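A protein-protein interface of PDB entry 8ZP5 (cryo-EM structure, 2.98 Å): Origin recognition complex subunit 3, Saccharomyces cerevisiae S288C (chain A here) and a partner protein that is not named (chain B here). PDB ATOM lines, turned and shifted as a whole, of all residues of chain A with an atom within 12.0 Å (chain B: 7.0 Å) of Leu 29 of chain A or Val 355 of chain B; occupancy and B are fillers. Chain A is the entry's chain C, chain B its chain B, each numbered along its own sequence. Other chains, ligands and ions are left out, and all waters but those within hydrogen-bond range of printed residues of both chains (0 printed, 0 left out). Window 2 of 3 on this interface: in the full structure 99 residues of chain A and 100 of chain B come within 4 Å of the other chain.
The side-chain hydroxyl (OG) of Ser 357 of chain B is in hydrogen-bond range of the backbone carbonyl oxygen (O) of Pro 27 of chain A (2.9 Å).
The backbone NH (N) of Leu 29 of chain A sits close to the side-chain hydroxyl (OG) of Ser 357 of chain B.
OH of Tyr 340 of chain B lies within hydrogen-bond range of O of Pro 30 of chain A (3.0 Å).
Among the printed residues, merely in contact across the chains: Pro 27 of chain A with Ser 335 of chain B (3.6 Å), Leu 29 of chain A with Tyr 340 of chain B (3.5 Å), Leu 29 of chain A with Val 355 of chain B (3.8 Å), Pro 30 of chain A with Pro 336 of chain B (3.9 Å), Lys 37 of chain A with Lys 337 of chain B (3.7 Å) and His 38 of chain A with Tyr 340 of chain B (3.5 Å).
Val 25 of chain A touches none of the printed residues of chain B.
Tyr 26 of chain A touches none of the printed residues of chain B.
Leu 29 of chain A touches just these residues of chain B: Tyr 340 (3.5 Å), Val 355 (3.8 Å) and Ser 357 (3.3 Å).
Of the printed residues of chain B, Pro 30 of chain A touches Pro 336 and Tyr 340.
Of the printed residues of chain A, Ser 335 of chain B touches Pro 27.
Pro 336 of chain B touches just one residue of chain A: Pro 30 (3.9 Å).
No residue of chain A comes within 4 Å of Ala 339 of chain B.
Tyr 340 of chain B touches just these residues of chain A: Leu 29 (3.5 Å), Pro 30 (3.0 Å) and His 38 (3.5 Å).
Val 355 of chain B touches one residue of chain A.
Asn 356 of chain B touches none of the printed residues of chain A.
The nearest residue of chain B that does not touch Leu 29 of chain A is Pro 336 of chain B (4.3 Å).
The nearest residue of chain A that does not touch Val 355 of chain B is Pro 27 of chain A (7.5 Å).
Of the 8 printed residues of chain A, 5 touch a printed residue of chain B.
Hydrophobic or aromatic side chains of chain A within 4 Å of the printed part of chain B: Pro 27, Leu 29, Pro 30 and His 38.
Hydrophobic or aromatic side chains of chain B that line the printed part of chain A: Pro 336, Tyr 340 and Val 355.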
ATOM      1  N   VAL A  25      -5.578  -9.522  -7.420  1.00  0.00           N
ATOM      2  CA  VAL A  25      -6.721  -8.923  -8.096  1.00  0.00           C
ATOM      3  C   VAL A  25      -6.788  -9.474  -9.511  1.00  0.00           C
ATOM      4  O   VAL A  25      -5.765  -9.550 -10.202  1.00  0.00           O
ATOM      5  CB  VAL A  25      -6.628  -7.386  -8.117  1.00  0.00           C
ATOM      6  CG1 VAL A  25      -7.851  -6.788  -8.793  1.00  0.00           C
ATOM      7  CG2 VAL A  25      -6.475  -6.845  -6.710  1.00  0.00           C
ATOM      8  N   TYR A  26      -7.987  -9.866  -9.938  1.00  0.00           N
ATOM      9  CA  TYR A  26      -8.231 -10.256 -11.323  1.00  0.00           C
ATOM     10  C   TYR A  26      -9.047  -9.159 -11.990  1.00  0.00           C
ATOM     11  O   TYR A  26     -10.269  -9.086 -11.790  1.00  0.00           O
ATOM     12  CB  TYR A  26      -8.969 -11.594 -11.398  1.00  0.00           C
ATOM     13  CG  TYR A  26      -8.156 -12.785 -10.948  1.00  0.00           C
ATOM     14  CD1 TYR A  26      -7.262 -13.405 -11.810  1.00  0.00           C
ATOM     15  CD2 TYR A  26      -8.291 -13.299  -9.666  1.00  0.00           C
ATOM     16  CE1 TYR A  26      -6.521 -14.496 -11.406  1.00  0.00           C
ATOM     17  CE2 TYR A  26      -7.554 -14.389  -9.254  1.00  0.00           C
ATOM     18  CZ  TYR A  26      -6.671 -14.985 -10.127  1.00  0.00           C
ATOM     19  OH  TYR A  26      -5.936 -16.072  -9.720  1.00  0.00           O
ATOM     20  N   PRO A  27      -8.429  -8.284 -12.778  1.00  0.00           N
ATOM     21  CA  PRO A  27      -9.174  -7.170 -13.371  1.00  0.00           C
ATOM     22  C   PRO A  27     -10.222  -7.648 -14.362  1.00  0.00           C
ATOM     23  O   PRO A  27     -10.076  -8.688 -15.009  1.00  0.00           O
ATOM     24  CB  PRO A  27      -8.086  -6.345 -14.069  1.00  0.00           C
ATOM     25  CG  PRO A  27      -6.809  -6.764 -13.416  1.00  0.00           C
ATOM     26  CD  PRO A  27      -6.992  -8.208 -13.083  1.00  0.00           C
ATOM     27  N   SER A  28     -11.294  -6.868 -14.470  1.00  0.00           N
ATOM     28  CA  SER A  28     -12.375  -7.135 -15.411  1.00  0.00           C
ATOM     29  C   SER A  28     -12.135  -6.295 -16.659  1.00  0.00           C
ATOM     30  O   SER A  28     -12.380  -5.084 -16.658  1.00  0.00           O
ATOM     31  CB  SER A  28     -13.733  -6.822 -14.786  1.00  0.00           C
ATOM     32  OG  SER A  28     -13.838  -5.447 -14.458  1.00  0.00           O
ATOM     33  N   LEU A  29     -11.652  -6.937 -17.717  1.00  0.00           N
ATOM     34  CA  LEU A  29     -11.360  -6.223 -18.949  1.00  0.00           C
ATOM     35  C   LEU A  29     -12.657  -5.745 -19.600  1.00  0.00           C
ATOM     36  O   LEU A  29     -13.687  -6.419 -19.504  1.00  0.00           O
ATOM     37  CB  LEU A  29     -10.577  -7.117 -19.915  1.00  0.00           C
ATOM     38  CG  LEU A  29     -11.298  -8.244 -20.661  1.00  0.00           C
ATOM     39  CD1 LEU A  29     -10.436  -8.738 -21.807  1.00  0.00           C
ATOM     40  CD2 LEU A  29     -11.655  -9.397 -19.736  1.00  0.00           C
ATOM     41  N   PRO A  30     -12.645  -4.573 -20.255  1.00  0.00           N
ATOM     42  CA  PRO A  30     -13.827  -3.996 -20.908  1.00  0.00           C
ATOM     43  C   PRO A  30     -14.420  -4.903 -21.982  1.00  0.00           C
ATOM     44  O   PRO A  30     -14.529  -4.474 -23.132  1.00  0.00           O
ATOM     45  CB  PRO A  30     -13.286  -2.705 -21.531  1.00  0.00           C
ATOM     46  CG  PRO A  30     -12.090  -2.365 -20.715  1.00  0.00           C
ATOM     47  CD  PRO A  30     -11.478  -3.678 -20.347  1.00  0.00           C
ATOM     48  N   LYS A  37      -5.762  -1.022 -31.198  1.00  0.00           N
ATOM     49  CA  LYS A  37      -5.099   0.012 -30.414  1.00  0.00           C
ATOM     50  C   LYS A  37      -4.170  -0.601 -29.373  1.00  0.00           C
ATOM     51  O   LYS A  37      -3.987  -0.038 -28.288  1.00  0.00           O
ATOM     52  CB  LYS A  37      -6.119   0.925 -29.730  1.00  0.00           C
ATOM     53  CG  LYS A  37      -7.241   0.182 -29.026  1.00  0.00           C
ATOM     54  CD  LYS A  37      -8.297   1.142 -28.503  1.00  0.00           C
ATOM     55  CE  LYS A  37      -9.406   0.399 -27.780  1.00  0.00           C
ATOM     56  NZ  LYS A  37      -9.785  -0.854 -28.488  1.00  0.00           N
ATOM     57  N   HIS A  38      -3.573  -1.749 -29.689  1.00  0.00           N
ATOM     58  CA  HIS A  38      -2.744  -2.493 -28.752  1.00  0.00           C
ATOM     59  C   HIS A  38      -1.260  -2.186 -28.914  1.00  0.00           C
ATOM     60  O   HIS A  38      -0.420  -2.902 -28.360  1.00  0.00           O
ATOM     61  CB  HIS A  38      -2.997  -3.991 -28.910  1.00  0.00           C
ATOM     62  CG  HIS A  38      -4.443  -4.341 -29.078  1.00  0.00           C
ATOM     63  ND1 HIS A  38      -4.914  -5.062 -30.153  1.00  0.00           N
ATOM     64  CD2 HIS A  38      -5.522  -4.063 -28.309  1.00  0.00           C
ATOM     65  CE1 HIS A  38      -6.222  -5.218 -30.038  1.00  0.00           C
ATOM     66  NE2 HIS A  38      -6.614  -4.621 -28.928  1.00  0.00           N
ATOM     67  N   SER B 335      -3.290  -4.208 -17.091  1.00  0.00           N
ATOM     68  CA  SER B 335      -3.782  -5.572 -17.279  1.00  0.00           C
ATOM     69  C   SER B 335      -4.726  -5.709 -18.467  1.00  0.00           C
ATOM     70  O   SER B 335      -4.513  -6.621 -19.286  1.00  0.00           O
ATOM     71  CB  SER B 335      -4.427  -6.068 -15.982  1.00  0.00           C
ATOM     72  OG  SER B 335      -3.475  -6.124 -14.935  1.00  0.00           O
ATOM     73  N   PRO B 336      -5.772  -4.886 -18.627  1.00  0.00           N
ATOM     74  CA  PRO B 336      -6.606  -5.010 -19.832  1.00  0.00           C
ATOM     75  C   PRO B 336      -5.845  -4.792 -21.126  1.00  0.00           C
ATOM     76  O   PRO B 336      -6.103  -5.506 -22.102  1.00  0.00           O
ATOM     77  CB  PRO B 336      -7.678  -3.931 -19.631  1.00  0.00           C
ATOM     78  CG  PRO B 336      -7.739  -3.746 -18.163  1.00  0.00           C
ATOM     79  CD  PRO B 336      -6.317  -3.865 -17.715  1.00  0.00           C
ATOM     80  N   LYS B 337      -4.906  -3.848 -21.164  1.00  0.00           N
ATOM     81  CA  LYS B 337      -4.147  -3.595 -22.382  1.00  0.00           C
ATOM     82  C   LYS B 337      -3.245  -4.765 -22.745  1.00  0.00           C
ATOM     83  O   LYS B 337      -3.175  -5.149 -23.918  1.00  0.00           O
ATOM     84  CB  LYS B 337      -3.321  -2.317 -22.236  1.00  0.00           C
ATOM     85  CG  LYS B 337      -4.154  -1.049 -22.287  1.00  0.00           C
ATOM     86  CD  LYS B 337      -4.407  -0.611 -23.717  1.00  0.00           C
ATOM     87  CE  LYS B 337      -5.270   0.638 -23.758  1.00  0.00           C
ATOM     88  NZ  LYS B 337      -5.296   1.247 -25.115  1.00  0.00           N
ATOM     89  N   ALA B 339      -3.818  -7.846 -21.841  1.00  0.00           N
ATOM     90  CA  ALA B 339      -4.726  -8.928 -22.208  1.00  0.00           C
ATOM     91  C   ALA B 339      -5.191  -8.792 -23.653  1.00  0.00           C
ATOM     92  O   ALA B 339      -5.235  -9.777 -24.397  1.00  0.00           O
ATOM     93  CB  ALA B 339      -5.921  -8.953 -21.256  1.00  0.00           C
ATOM     94  N   TYR B 340      -5.545  -7.574 -24.070  1.00  0.00           N
ATOM     95  CA  TYR B 340      -5.962  -7.370 -25.455  1.00  0.00           C
ATOM     96  C   TYR B 340      -4.799  -7.515 -26.427  1.00  0.00           C
ATOM     97  O   TYR B 340      -4.989  -8.023 -27.539  1.00  0.00           O
ATOM     98  CB  TYR B 340      -6.627  -6.005 -25.625  1.00  0.00           C
ATOM     99  CG  TYR B 340      -7.980  -5.893 -24.964  1.00  0.00           C
ATOM    100  CD1 TYR B 340      -8.255  -4.878 -24.059  1.00  0.00           C
ATOM    101  CD2 TYR B 340      -8.987  -6.803 -25.251  1.00  0.00           C
ATOM    102  CE1 TYR B 340      -9.491  -4.775 -23.456  1.00  0.00           C
ATOM    103  CE2 TYR B 340     -10.226  -6.707 -24.655  1.00  0.00           C
ATOM    104  CZ  TYR B 340     -10.472  -5.692 -23.758  1.00  0.00           C
ATOM    105  OH  TYR B 340     -11.706  -5.594 -23.160  1.00  0.00           O
ATOM    106  N   GLN B 342      -2.349  -9.521 -26.091  1.00  0.00           N
ATOM    107  CA  GLN B 342      -1.941 -10.919 -26.134  1.00  0.00           C
ATOM    108  C   GLN B 342      -3.074 -11.804 -26.642  1.00  0.00           C
ATOM    109  O   GLN B 342      -3.653 -11.541 -27.697  1.00  0.00           O
ATOM    110  CB  GLN B 342      -1.487 -11.389 -24.751  1.00  0.00           C
ATOM    111  CG  GLN B 342      -0.081 -10.957 -24.383  1.00  0.00           C
ATOM    112  CD  GLN B 342       0.326 -11.427 -23.004  1.00  0.00           C
ATOM    113  OE1 GLN B 342       1.334 -10.982 -22.457  1.00  0.00           O
ATOM    114  NE2 GLN B 342      -0.458 -12.333 -22.433  1.00  0.00           N
ATOM    115  N   VAL B 355     -11.390 -14.831 -23.117  1.00  0.00           N
ATOM    116  CA  VAL B 355     -10.249 -13.980 -22.808  1.00  0.00           C
ATOM    117  C   VAL B 355     -10.325 -13.520 -21.353  1.00  0.00           C
ATOM    118  O   VAL B 355     -11.408 -13.259 -20.829  1.00  0.00           O
ATOM    119  CB  VAL B 355     -10.173 -12.777 -23.779  1.00  0.00           C
ATOM    120  CG1 VAL B 355     -11.390 -11.876 -23.627  1.00  0.00           C
ATOM    121  CG2 VAL B 355      -8.884 -11.993 -23.571  1.00  0.00           C
ATOM    122  N   ASN B 356      -9.168 -13.446 -20.696  1.00  0.00           N
ATOM    123  CA  ASN B 356      -9.090 -13.010 -19.312  1.00  0.00           C
ATOM    124  C   ASN B 356      -7.922 -12.051 -19.148  1.00  0.00           C
ATOM    125  O   ASN B 356      -6.942 -12.107 -19.895  1.00  0.00           O
ATOM    126  CB  ASN B 356      -8.935 -14.195 -18.350  1.00  0.00           C
ATOM    127  CG  ASN B 356      -9.360 -13.856 -16.936  1.00  0.00           C
ATOM    128  OD1 ASN B 356     -10.388 -13.214 -16.721  1.00  0.00           O
ATOM    129  ND2 ASN B 356      -8.566 -14.283 -15.961  1.00  0.00           N
ATOM    130  N   SER B 357      -8.037 -11.168 -18.160  1.00  0.00           N
ATOM    131  CA  SER B 357      -7.000 -10.189 -17.890  1.00  0.00           C
ATOM    132  C   SER B 357      -5.839 -10.825 -17.133  1.00  0.00           C
ATOM    133  O   SER B 357      -5.974 -11.874 -16.497  1.00  0.00           O
ATOM    134  CB  SER B 357      -7.561  -9.014 -17.091  1.00  0.00           C
ATOM    135  OG  SER B 357      -8.806  -8.591 -17.617  1.00  0.00           O
